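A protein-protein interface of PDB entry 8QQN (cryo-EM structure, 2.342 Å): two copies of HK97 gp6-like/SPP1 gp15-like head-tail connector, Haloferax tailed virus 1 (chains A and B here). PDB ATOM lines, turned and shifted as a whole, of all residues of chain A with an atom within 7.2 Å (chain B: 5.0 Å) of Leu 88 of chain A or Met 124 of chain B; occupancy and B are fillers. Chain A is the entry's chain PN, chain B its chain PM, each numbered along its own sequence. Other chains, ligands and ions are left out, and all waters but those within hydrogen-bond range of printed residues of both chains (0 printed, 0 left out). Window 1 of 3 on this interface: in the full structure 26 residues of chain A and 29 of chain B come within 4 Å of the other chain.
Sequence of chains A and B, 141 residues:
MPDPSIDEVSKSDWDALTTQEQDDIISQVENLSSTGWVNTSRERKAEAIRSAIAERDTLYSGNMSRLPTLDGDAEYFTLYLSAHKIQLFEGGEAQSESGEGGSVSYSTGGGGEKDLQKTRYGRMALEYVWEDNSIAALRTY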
ATOM      1  N   TRP A  37      28.636 -18.776   7.323  1.00  0.00           N
ATOM      2  CA  TRP A  37      27.490 -18.421   6.485  1.00  0.00           C
ATOM      3  C   TRP A  37      26.563 -17.416   7.184  1.00  0.00           C
ATOM      4  O   TRP A  37      25.340 -17.594   7.196  1.00  0.00           O
ATOM      5  CB  TRP A  37      26.730 -19.672   6.014  1.00  0.00           C
ATOM      6  CG  TRP A  37      27.564 -20.727   5.353  1.00  0.00           C
ATOM      7  CD1 TRP A  37      28.034 -20.712   4.071  1.00  0.00           C
ATOM      8  CD2 TRP A  37      28.011 -21.978   5.925  1.00  0.00           C
ATOM      9  NE1 TRP A  37      28.736 -21.861   3.814  1.00  0.00           N
ATOM     10  CE2 TRP A  37      28.742 -22.667   4.928  1.00  0.00           C
ATOM     11  CE3 TRP A  37      27.875 -22.587   7.179  1.00  0.00           C
ATOM     12  CZ2 TRP A  37      29.338 -23.918   5.165  1.00  0.00           C
ATOM     13  CZ3 TRP A  37      28.457 -23.819   7.419  1.00  0.00           C
ATOM     14  CH2 TRP A  37      29.178 -24.479   6.419  1.00  0.00           C
ATOM     15  N   SER A  51      16.905 -31.370   6.106  1.00  0.00           N
ATOM     16  CA  SER A  51      17.124 -32.079   4.856  1.00  0.00           C
ATOM     17  C   SER A  51      18.269 -33.094   4.952  1.00  0.00           C
ATOM     18  O   SER A  51      18.138 -34.207   4.455  1.00  0.00           O
ATOM     19  CB  SER A  51      17.334 -31.107   3.740  1.00  0.00           C
ATOM     20  OG  SER A  51      17.379 -31.789   2.501  1.00  0.00           O
ATOM     21  N   GLU A  55      17.915 -37.120   4.640  1.00  0.00           N
ATOM     22  CA  GLU A  55      18.706 -37.751   3.597  1.00  0.00           C
ATOM     23  C   GLU A  55      19.636 -38.835   4.154  1.00  0.00           C
ATOM     24  O   GLU A  55      19.796 -39.878   3.527  1.00  0.00           O
ATOM     25  CB  GLU A  55      19.462 -36.656   2.860  1.00  0.00           C
ATOM     26  CG  GLU A  55      20.092 -37.143   1.589  1.00  0.00           C
ATOM     27  CD  GLU A  55      20.546 -36.013   0.684  1.00  0.00           C
ATOM     28  OE1 GLU A  55      19.735 -35.099   0.416  1.00  0.00           O
ATOM     29  OE2 GLU A  55      21.721 -36.018   0.272  1.00  0.00           O
ATOM     30  N   LEU A  59      18.657 -42.188   2.369  1.00  0.00           N
ATOM     31  CA  LEU A  59      19.601 -42.562   1.315  1.00  0.00           C
ATOM     32  C   LEU A  59      20.891 -43.200   1.837  1.00  0.00           C
ATOM     33  O   LEU A  59      21.556 -43.913   1.087  1.00  0.00           O
ATOM     34  CB  LEU A  59      19.923 -41.348   0.440  1.00  0.00           C
ATOM     35  CG  LEU A  59      18.744 -40.783  -0.347  1.00  0.00           C
ATOM     36  CD1 LEU A  59      19.185 -39.620  -1.219  1.00  0.00           C
ATOM     37  CD2 LEU A  59      18.105 -41.870  -1.197  1.00  0.00           C
ATOM     38  N   SER A  82      25.050 -31.398   6.036  1.00  0.00           N
ATOM     39  CA  SER A  82      24.389 -30.124   6.314  1.00  0.00           C
ATOM     40  C   SER A  82      25.164 -28.945   5.722  1.00  0.00           C
ATOM     41  O   SER A  82      24.579 -28.090   5.066  1.00  0.00           O
ATOM     42  CB  SER A  82      24.175 -29.922   7.794  1.00  0.00           C
ATOM     43  OG  SER A  82      23.457 -31.005   8.354  1.00  0.00           O
ATOM     44  N   ALA A  83      26.486 -28.908   5.932  1.00  0.00           N
ATOM     45  CA  ALA A  83      27.388 -27.905   5.377  1.00  0.00           C
ATOM     46  C   ALA A  83      27.381 -27.918   3.842  1.00  0.00           C
ATOM     47  O   ALA A  83      27.301 -26.860   3.221  1.00  0.00           O
ATOM     48  CB  ALA A  83      28.768 -28.114   5.950  1.00  0.00           C
ATOM     49  N   HIS A  84      27.383 -29.111   3.228  1.00  0.00           N
ATOM     50  CA  HIS A  84      27.242 -29.278   1.784  1.00  0.00           C
ATOM     51  C   HIS A  84      25.977 -28.592   1.269  1.00  0.00           C
ATOM     52  O   HIS A  84      26.047 -27.804   0.333  1.00  0.00           O
ATOM     53  CB  HIS A  84      27.311 -30.764   1.401  1.00  0.00           C
ATOM     54  CG  HIS A  84      26.948 -31.060  -0.021  1.00  0.00           C
ATOM     55  ND1 HIS A  84      27.727 -30.730  -1.132  1.00  0.00           N
ATOM     56  CD2 HIS A  84      25.829 -31.627  -0.511  1.00  0.00           C
ATOM     57  CE1 HIS A  84      27.102 -31.125  -2.234  1.00  0.00           C
ATOM     58  NE2 HIS A  84      25.942 -31.670  -1.874  1.00  0.00           N
ATOM     59  N   LYS A  85      24.843 -28.826   1.937  1.00  0.00           N
ATOM     60  CA  LYS A  85      23.567 -28.224   1.583  1.00  0.00           C
ATOM     61  C   LYS A  85      23.583 -26.704   1.724  1.00  0.00           C
ATOM     62  O   LYS A  85      23.218 -26.030   0.772  1.00  0.00           O
ATOM     63  CB  LYS A  85      22.432 -28.911   2.333  1.00  0.00           C
ATOM     64  CG  LYS A  85      22.206 -30.311   1.796  1.00  0.00           C
ATOM     65  CD  LYS A  85      21.098 -31.067   2.467  1.00  0.00           C
ATOM     66  CE  LYS A  85      20.950 -32.487   1.960  1.00  0.00           C
ATOM     67  NZ  LYS A  85      20.698 -32.546   0.499  1.00  0.00           N
ATOM     68  N   ILE A  86      24.087 -26.154   2.839  1.00  0.00           N
ATOM     69  CA  ILE A  86      24.166 -24.707   3.038  1.00  0.00           C
ATOM     70  C   ILE A  86      25.003 -24.047   1.936  1.00  0.00           C
ATOM     71  O   ILE A  86      24.592 -23.031   1.370  1.00  0.00           O
ATOM     72  CB  ILE A  86      24.651 -24.344   4.460  1.00  0.00           C
ATOM     73  CG1 ILE A  86      23.677 -24.841   5.531  1.00  0.00           C
ATOM     74  CG2 ILE A  86      24.869 -22.842   4.603  1.00  0.00           C
ATOM     75  CD1 ILE A  86      24.281 -24.986   6.908  1.00  0.00           C
ATOM     76  N   GLN A  87      26.146 -24.648   1.585  1.00  0.00           N
ATOM     77  CA  GLN A  87      27.010 -24.149   0.523  1.00  0.00           C
ATOM     78  C   GLN A  87      26.330 -24.199  -0.854  1.00  0.00           C
ATOM     79  O   GLN A  87      26.524 -23.303  -1.670  1.00  0.00           O
ATOM     80  CB  GLN A  87      28.346 -24.891   0.538  1.00  0.00           C
ATOM     81  CG  GLN A  87      29.403 -24.233  -0.346  1.00  0.00           C
ATOM     82  CD  GLN A  87      29.806 -22.860   0.142  1.00  0.00           C
ATOM     83  OE1 GLN A  87      30.112 -22.679   1.316  1.00  0.00           O
ATOM     84  NE2 GLN A  87      29.803 -21.866  -0.734  1.00  0.00           N
ATOM     85  N   LEU A  88      25.509 -25.221  -1.126  1.00  0.00           N
ATOM     86  CA  LEU A  88      24.701 -25.246  -2.338  1.00  0.00           C
ATOM     87  C   LEU A  88      23.595 -24.185  -2.323  1.00  0.00           C
ATOM     88  O   LEU A  88      23.314 -23.612  -3.369  1.00  0.00           O
ATOM     89  CB  LEU A  88      24.139 -26.647  -2.598  1.00  0.00           C
ATOM     90  CG  LEU A  88      25.149 -27.728  -2.990  1.00  0.00           C
ATOM     91  CD1 LEU A  88      24.404 -28.966  -3.433  1.00  0.00           C
ATOM     92  CD2 LEU A  88      26.075 -27.261  -4.107  1.00  0.00           C
ATOM     93  N   PHE A  89      23.010 -23.859  -1.160  1.00  0.00           N
ATOM     94  CA  PHE A  89      22.028 -22.784  -1.048  1.00  0.00           C
ATOM     95  C   PHE A  89      22.654 -21.399  -1.279  1.00  0.00           C
ATOM     96  O   PHE A  89      21.961 -20.474  -1.710  1.00  0.00           O
ATOM     97  CB  PHE A  89      21.310 -22.840   0.307  1.00  0.00           C
ATOM     98  CG  PHE A  89      20.545 -24.093   0.693  1.00  0.00           C
ATOM     99  CD1 PHE A  89      20.425 -25.200  -0.143  1.00  0.00           C
ATOM    100  CD2 PHE A  89      19.886 -24.140   1.918  1.00  0.00           C
ATOM    101  CE1 PHE A  89      19.710 -26.328   0.252  1.00  0.00           C
ATOM    102  CE2 PHE A  89      19.164 -25.261   2.310  1.00  0.00           C
ATOM    103  CZ  PHE A  89      19.087 -26.360   1.484  1.00  0.00           C
ATOM    104  N   GLU A  90      23.964 -21.264  -1.013  1.00  0.00           N
ATOM    105  CA  GLU A  90      24.781 -20.082  -1.272  1.00  0.00           C
ATOM    106  C   GLU A  90      25.185 -19.936  -2.751  1.00  0.00           C
ATOM    107  O   GLU A  90      25.856 -18.965  -3.110  1.00  0.00           O
ATOM    108  CB  GLU A  90      26.023 -20.141  -0.376  1.00  0.00           C
ATOM    109  CG  GLU A  90      25.724 -19.924   1.098  1.00  0.00           C
ATOM    110  CD  GLU A  90      25.723 -18.471   1.542  1.00  0.00           C
ATOM    111  OE1 GLU A  90      25.783 -17.576   0.672  1.00  0.00           O
ATOM    112  OE2 GLU A  90      25.668 -18.224   2.767  1.00  0.00           O
ATOM    113  N   GLY A  91      24.815 -20.887  -3.622  1.00  0.00           N
ATOM    114  CA  GLY A  91      25.088 -20.810  -5.052  1.00  0.00           C
ATOM    115  C   GLY A  91      26.134 -21.812  -5.548  1.00  0.00           C
ATOM    116  O   GLY A  91      26.373 -21.902  -6.751  1.00  0.00           O
ATOM    117  N   GLY A  92      26.750 -22.564  -4.625  1.00  0.00           N
ATOM    118  CA  GLY A  92      27.795 -23.525  -4.944  1.00  0.00           C
ATOM    119  C   GLY A  92      29.137 -23.163  -4.312  1.00  0.00           C
ATOM    120  O   GLY A  92      29.259 -22.205  -3.546  1.00  0.00           O
ATOM    121  N   GLU A  93      30.152 -23.969  -4.620  1.00  0.00           N
ATOM    122  CA  GLU A  93      31.516 -23.729  -4.170  1.00  0.00           C
ATOM    123  C   GLU A  93      32.187 -22.662  -5.044  1.00  0.00           C
ATOM    124  O   GLU A  93      32.163 -22.754  -6.274  1.00  0.00           O
ATOM    125  CB  GLU A  93      32.248 -25.070  -4.197  1.00  0.00           C
ATOM    126  CG  GLU A  93      33.693 -25.038  -3.740  1.00  0.00           C
ATOM    127  CD  GLU A  93      34.030 -26.291  -2.951  1.00  0.00           C
ATOM    128  OE1 GLU A  93      33.632 -26.355  -1.762  1.00  0.00           O
ATOM    129  OE2 GLU A  93      34.617 -27.237  -3.531  1.00  0.00           O
ATOM    130  N   LYS A 114      28.777 -35.606  -9.880  1.00  0.00           N
ATOM    131  CA  LYS A 114      27.699 -35.968  -8.964  1.00  0.00           C
ATOM    132  C   LYS A 114      27.561 -34.970  -7.815  1.00  0.00           C
ATOM    133  O   LYS A 114      28.485 -34.221  -7.510  1.00  0.00           O
ATOM    134  CB  LYS A 114      27.914 -37.393  -8.456  1.00  0.00           C
ATOM    135  CG  LYS A 114      27.879 -38.421  -9.572  1.00  0.00           C
ATOM    136  CD  LYS A 114      28.186 -39.816  -9.105  1.00  0.00           C
ATOM    137  CE  LYS A 114      28.199 -40.825 -10.235  1.00  0.00           C
ATOM    138  NZ  LYS A 114      26.830 -41.161 -10.696  1.00  0.00           N
ATOM    139  N   ASP A 115      26.400 -35.008  -7.151  1.00  0.00           N
ATOM    140  CA  ASP A 115      26.021 -34.124  -6.055  1.00  0.00           C
ATOM    141  C   ASP A 115      27.138 -33.905  -5.021  1.00  0.00           C
ATOM    142  O   ASP A 115      27.656 -32.794  -4.888  1.00  0.00           O
ATOM    143  CB  ASP A 115      24.727 -34.630  -5.419  1.00  0.00           C
ATOM    144  CG  ASP A 115      24.308 -33.866  -4.175  1.00  0.00           C
ATOM    145  OD1 ASP A 115      24.656 -32.674  -4.075  1.00  0.00           O
ATOM    146  OD2 ASP A 115      23.636 -34.468  -3.311  1.00  0.00           O
ATOM    147  N   LEU A 116      27.534 -34.956  -4.290  1.00  0.00           N
ATOM    148  CA  LEU A 116      28.480 -34.791  -3.192  1.00  0.00           C
ATOM    149  C   LEU A 116      29.890 -34.424  -3.678  1.00  0.00           C
ATOM    150  O   LEU A 116      30.636 -33.785  -2.953  1.00  0.00           O
ATOM    151  CB  LEU A 116      28.477 -36.026  -2.285  1.00  0.00           C
ATOM    152  CG  LEU A 116      27.225 -36.282  -1.441  1.00  0.00           C
ATOM    153  CD1 LEU A 116      27.421 -37.523  -0.585  1.00  0.00           C
ATOM    154  CD2 LEU A 116      26.887 -35.103  -0.542  1.00  0.00           C
ATOM    155  N   LYS A 118      30.623 -32.119  -5.739  1.00  0.00           N
ATOM    156  CA  LYS A 118      30.605 -30.732  -6.197  1.00  0.00           C
ATOM    157  C   LYS A 118      30.984 -29.684  -5.141  1.00  0.00           C
ATOM    158  O   LYS A 118      31.222 -28.537  -5.512  1.00  0.00           O
ATOM    159  CB  LYS A 118      29.274 -30.417  -6.889  1.00  0.00           C
ATOM    160  CG  LYS A 118      29.229 -30.745  -8.376  1.00  0.00           C
ATOM    161  CD  LYS A 118      29.740 -29.600  -9.240  1.00  0.00           C
ATOM    162  CE  LYS A 118      29.820 -29.925 -10.717  1.00  0.00           C
ATOM    163  NZ  LYS A 118      31.174 -30.382 -11.115  1.00  0.00           N
ATOM    164  N   THR A 119      31.067 -30.039  -3.846  1.00  0.00           N
ATOM    165  CA  THR A 119      31.650 -29.141  -2.844  1.00  0.00           C
ATOM    166  C   THR A 119      32.561 -29.904  -1.878  1.00  0.00           C
ATOM    167  O   THR A 119      32.407 -31.106  -1.701  1.00  0.00           O
ATOM    168  CB  THR A 119      30.621 -28.261  -2.104  1.00  0.00           C
ATOM    169  OG1 THR A 119      30.053 -28.908  -0.970  1.00  0.00           O
ATOM    170  CG2 THR A 119      29.467 -27.751  -2.938  1.00  0.00           C
ATOM    171  N   TYR B  80      13.425 -29.988  -3.885  1.00  0.00           N
ATOM    172  CA  TYR B  80      14.587 -29.836  -4.753  1.00  0.00           C
ATOM    173  C   TYR B  80      14.192 -29.765  -6.226  1.00  0.00           C
ATOM    174  O   TYR B  80      14.743 -28.964  -6.969  1.00  0.00           O
ATOM    175  CB  TYR B  80      15.602 -30.960  -4.533  1.00  0.00           C
ATOM    176  CG  TYR B  80      16.360 -30.870  -3.234  1.00  0.00           C
ATOM    177  CD1 TYR B  80      16.931 -29.673  -2.823  1.00  0.00           C
ATOM    178  CD2 TYR B  80      16.519 -31.981  -2.417  1.00  0.00           C
ATOM    179  CE1 TYR B  80      17.614 -29.568  -1.622  1.00  0.00           C
ATOM    180  CE2 TYR B  80      17.206 -31.891  -1.216  1.00  0.00           C
ATOM    181  CZ  TYR B  80      17.762 -30.686  -0.821  1.00  0.00           C
ATOM    182  OH  TYR B  80      18.447 -30.603   0.356  1.00  0.00           O
ATOM    183  N   ARG B 120      22.446 -27.445  -9.449  1.00  0.00           N
ATOM    184  CA  ARG B 120      22.783 -28.047  -8.162  1.00  0.00           C
ATOM    185  C   ARG B 120      21.588 -28.709  -7.462  1.00  0.00           C
ATOM    186  O   ARG B 120      21.743 -29.756  -6.833  1.00  0.00           O
ATOM    187  CB  ARG B 120      23.491 -27.010  -7.284  1.00  0.00           C
ATOM    188  CG  ARG B 120      22.624 -25.840  -6.844  1.00  0.00           C
ATOM    189  CD  ARG B 120      23.465 -24.632  -6.499  1.00  0.00           C
ATOM    190  NE  ARG B 120      22.690 -23.482  -6.068  1.00  0.00           N
ATOM    191  CZ  ARG B 120      22.221 -22.520  -6.854  1.00  0.00           C
ATOM    192  NH1 ARG B 120      21.570 -21.504  -6.316  1.00  0.00           N
ATOM    193  NH2 ARG B 120      22.381 -22.563  -8.162  1.00  0.00           N
ATOM    194  N   TYR B 121      20.397 -28.120  -7.594  1.00  0.00           N
ATOM    195  CA  TYR B 121      19.174 -28.678  -7.039  1.00  0.00           C
ATOM    196  C   TYR B 121      18.766 -29.964  -7.752  1.00  0.00           C
ATOM    197  O   TYR B 121      18.295 -30.900  -7.115  1.00  0.00           O
ATOM    198  CB  TYR B 121      18.066 -27.629  -7.076  1.00  0.00           C
ATOM    199  CG  TYR B 121      18.443 -26.367  -6.353  1.00  0.00           C
ATOM    200  CD1 TYR B 121      18.614 -26.389  -4.976  1.00  0.00           C
ATOM    201  CD2 TYR B 121      18.667 -25.172  -7.026  1.00  0.00           C
ATOM    202  CE1 TYR B 121      18.999 -25.259  -4.278  1.00  0.00           C
ATOM    203  CE2 TYR B 121      19.058 -24.027  -6.340  1.00  0.00           C
ATOM    204  CZ  TYR B 121      19.217 -24.076  -4.962  1.00  0.00           C
ATOM    205  OH  TYR B 121      19.599 -22.972  -4.262  1.00  0.00           O
ATOM    206  N   GLY B 122      18.970 -30.023  -9.067  1.00  0.00           N
ATOM    207  CA  GLY B 122      18.678 -31.215  -9.849  1.00  0.00           C
ATOM    208  C   GLY B 122      19.640 -32.357  -9.537  1.00  0.00           C
ATOM    209  O   GLY B 122      19.216 -33.502  -9.440  1.00  0.00           O
ATOM    210  N   ARG B 123      20.916 -32.031  -9.298  1.00  0.00           N
ATOM    211  CA  ARG B 123      21.930 -32.996  -8.896  1.00  0.00           C
ATOM    212  C   ARG B 123      21.598 -33.605  -7.533  1.00  0.00           C
ATOM    213  O   ARG B 123      21.682 -34.818  -7.380  1.00  0.00           O
ATOM    214  CB  ARG B 123      23.325 -32.376  -8.988  1.00  0.00           C
ATOM    215  CG  ARG B 123      23.729 -32.073 -10.423  1.00  0.00           C
ATOM    216  CD  ARG B 123      25.147 -31.562 -10.593  1.00  0.00           C
ATOM    217  NE  ARG B 123      25.456 -30.262 -10.007  1.00  0.00           N
ATOM    218  CZ  ARG B 123      25.482 -29.087 -10.630  1.00  0.00           C
ATOM    219  NH1 ARG B 123      25.845 -28.008  -9.963  1.00  0.00           N
ATOM    220  NH2 ARG B 123      25.124 -28.967 -11.893  1.00  0.00           N
ATOM    221  N   MET B 124      21.137 -32.791  -6.579  1.00  0.00           N
ATOM    222  CA  MET B 124      20.600 -33.283  -5.316  1.00  0.00           C
ATOM    223  C   MET B 124      19.369 -34.173  -5.518  1.00  0.00           C
ATOM    224  O   MET B 124      19.307 -35.245  -4.930  1.00  0.00           O
ATOM    225  CB  MET B 124      20.271 -32.133  -4.364  1.00  0.00           C
ATOM    226  CG  MET B 124      21.518 -31.541  -3.757  1.00  0.00           C
ATOM    227  SD  MET B 124      21.192 -30.358  -2.436  1.00  0.00           S
ATOM    228  CE  MET B 124      20.577 -28.961  -3.377  1.00  0.00           C
ATOM    229  N   ALA B 125      18.413 -33.765  -6.361  1.00  0.00           N
ATOM    230  CA  ALA B 125      17.201 -34.526  -6.651  1.00  0.00           C
ATOM    231  C   ALA B 125      17.496 -35.906  -7.259  1.00  0.00           C
ATOM    232  O   ALA B 125      16.841 -36.886  -6.907  1.00  0.00           O
ATOM    233  CB  ALA B 125      16.287 -33.691  -7.517  1.00  0.00           C
ATOM    234  N   LEU B 126      18.509 -36.015  -8.132  1.00  0.00           N
ATOM    235  CA  LEU B 126      18.904 -37.268  -8.768  1.00  0.00           C
ATOM    236  C   LEU B 126      19.264 -38.359  -7.759  1.00  0.00           C
ATOM    237  O   LEU B 126      18.949 -39.520  -7.989  1.00  0.00           O
ATOM    238  CB  LEU B 126      20.069 -37.029  -9.730  1.00  0.00           C
ATOM    239  CG  LEU B 126      19.662 -36.612 -11.140  1.00  0.00           C
ATOM    240  CD1 LEU B 126      20.837 -36.000 -11.884  1.00  0.00           C
ATOM    241  CD2 LEU B 126      19.074 -37.784 -11.924  1.00  0.00           C
ATOM    242  N   GLU B 127      19.880 -38.002  -6.629  1.00  0.00           N
ATOM    243  CA  GLU B 127      20.284 -38.958  -5.606  1.00  0.00           C
ATOM    244  C   GLU B 127      19.087 -39.659  -4.953  1.00  0.00           C
ATOM    245  O   GLU B 127      19.213 -40.795  -4.506  1.00  0.00           O
ATOM    246  CB  GLU B 127      21.166 -38.266  -4.565  1.00  0.00           C
ATOM    247  CG  GLU B 127      22.595 -38.009  -5.042  1.00  0.00           C
ATOM    248  CD  GLU B 127      23.543 -39.205  -5.101  1.00  0.00           C
ATOM    249  OE1 GLU B 127      23.172 -40.302  -4.622  1.00  0.00           O
ATOM    250  OE2 GLU B 127      24.658 -39.070  -5.650  1.00  0.00           O
ATOM    251  N   TYR B 128      17.918 -39.002  -4.924  1.00  0.00           N
ATOM    252  CA  TYR B 128      16.697 -39.532  -4.322  1.00  0.00           C
ATOM    253  C   TYR B 128      16.013 -40.574  -5.208  1.00  0.00           C
ATOM    254  O   TYR B 128      15.147 -41.314  -4.744  1.00  0.00           O
ATOM    255  CB  TYR B 128      15.710 -38.393  -4.046  1.00  0.00           C
ATOM    256  CG  TYR B 128      16.066 -37.508  -2.876  1.00  0.00           C
ATOM    257  CD1 TYR B 128      17.236 -36.755  -2.881  1.00  0.00           C
ATOM    258  CD2 TYR B 128      15.236 -37.411  -1.764  1.00  0.00           C
ATOM    259  CE1 TYR B 128      17.584 -35.954  -1.799  1.00  0.00           C
ATOM    260  CE2 TYR B 128      15.576 -36.622  -0.672  1.00  0.00           C
ATOM    261  CZ  TYR B 128      16.757 -35.897  -0.690  1.00  0.00           C
ATOM    262  OH  TYR B 128      17.119 -35.142   0.390  1.00  0.00           O
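The guanidinium group (NH1) of Arg 120 of chain B sits at hydrogen-bond distance from the side-chain hydroxyl (OH) of Tyr 121 of chain B (3.2 Å). The side-chain carboxylate (OD1) of Asp 115 of chain A lies within hydrogen-bond range of a ring nitrogen (NE2) of His 84 of chain A (2.7 Å). The side-chain carboxylate of Glu 55 of chain A lies within salt-bridge range of the side-chain amino group of Lys 85 of chain A (2.7 Å).
Of the printed residues of chain B, Glu 55 of chain A touches Tyr 128 (2.6 Å). Phe 89 of chain A touches none of the printed residues of chain B. Of the printed residues of chain B, Asp 115 of chain A touches Arg 123 (3.6 Å) and Met 124 (3.4 Å). Printed residues of chain A within 4 Å of Tyr 121 of chain B: Leu 88. Of chain A, only Lys 85 (3.7 Å), Leu 88 (3.6 Å) and Asp 115 (3.4 Å) come within 4 Å of Met 124 of chain B. The nearest residue of chain A that does not touch Met 124 of chain B is Phe 89 of chain A (4.6 Å). The nearest printed residue of chain B that does not touch Leu 59 of chain A is Met 124 of chain B (5.7 Å).
The side-chain amino group (NZ) of Lys 85 of chain A sits at hydrogen-bond distance from the side-chain sulfur (SD) of Met 124 of chain B. O of Leu 88 of chain A is in hydrogen-bond range of NE of Arg 120 of chain B (2.8 Å). OH of Tyr 80 of chain B sits at hydrogen-bond distance from NZ of Lys 85 of chain A (3.0 Å). The side-chain hydroxyl (OG) of Ser 51 of chain A is in hydrogen-bond range of the side-chain hydroxyl (OH) of Tyr 80 of chain B (2.7 Å). The side-chain carboxylate (OE1) of Glu 55 of chain A sits at hydrogen-bond distance from the side-chain hydroxyl (OH) of Tyr 128 of chain B, 2.6 Å away.
No position is printed for both chains. Of the 13 pairs that touch across the chains among the printed residues, none has its exchanged pair printed and touching as well.
Of the 21 printed residues of chain A, 7 touch a printed residue of chain B. Of the 10 printed residues of chain B, 7 touch a printed residue of chain A. Hydrophobic or aromatic side chains of chain B that line the printed part of chain A: Tyr 80, Tyr 121, Met 124 and Tyr 128. Among the printed residues, 13 pairs touch across the chains.
OG of Ser 51 of chain A touches OH of Tyr 128 of chain B, at 3.97 Å. Glu 127 of chain B touches Leu 59 of chain A. Tyr 128 of chain B touches Leu 59 of chain A (CD1 to CD1, 3.8 Å). O of Leu 88 of chain A touches OH of Tyr 121 of chain B (3.9 Å). Leu 88 of chain A touches Met 124 of chain B (CD1 to SD, 3.6 Å). Arg 120 of chain B touches Gly 91 of chain A. Asp 115 of chain A touches Arg 123 of chain B (CB to O, 3.6 Å). Asp 115 of chain A touches Met 124 of chain B.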
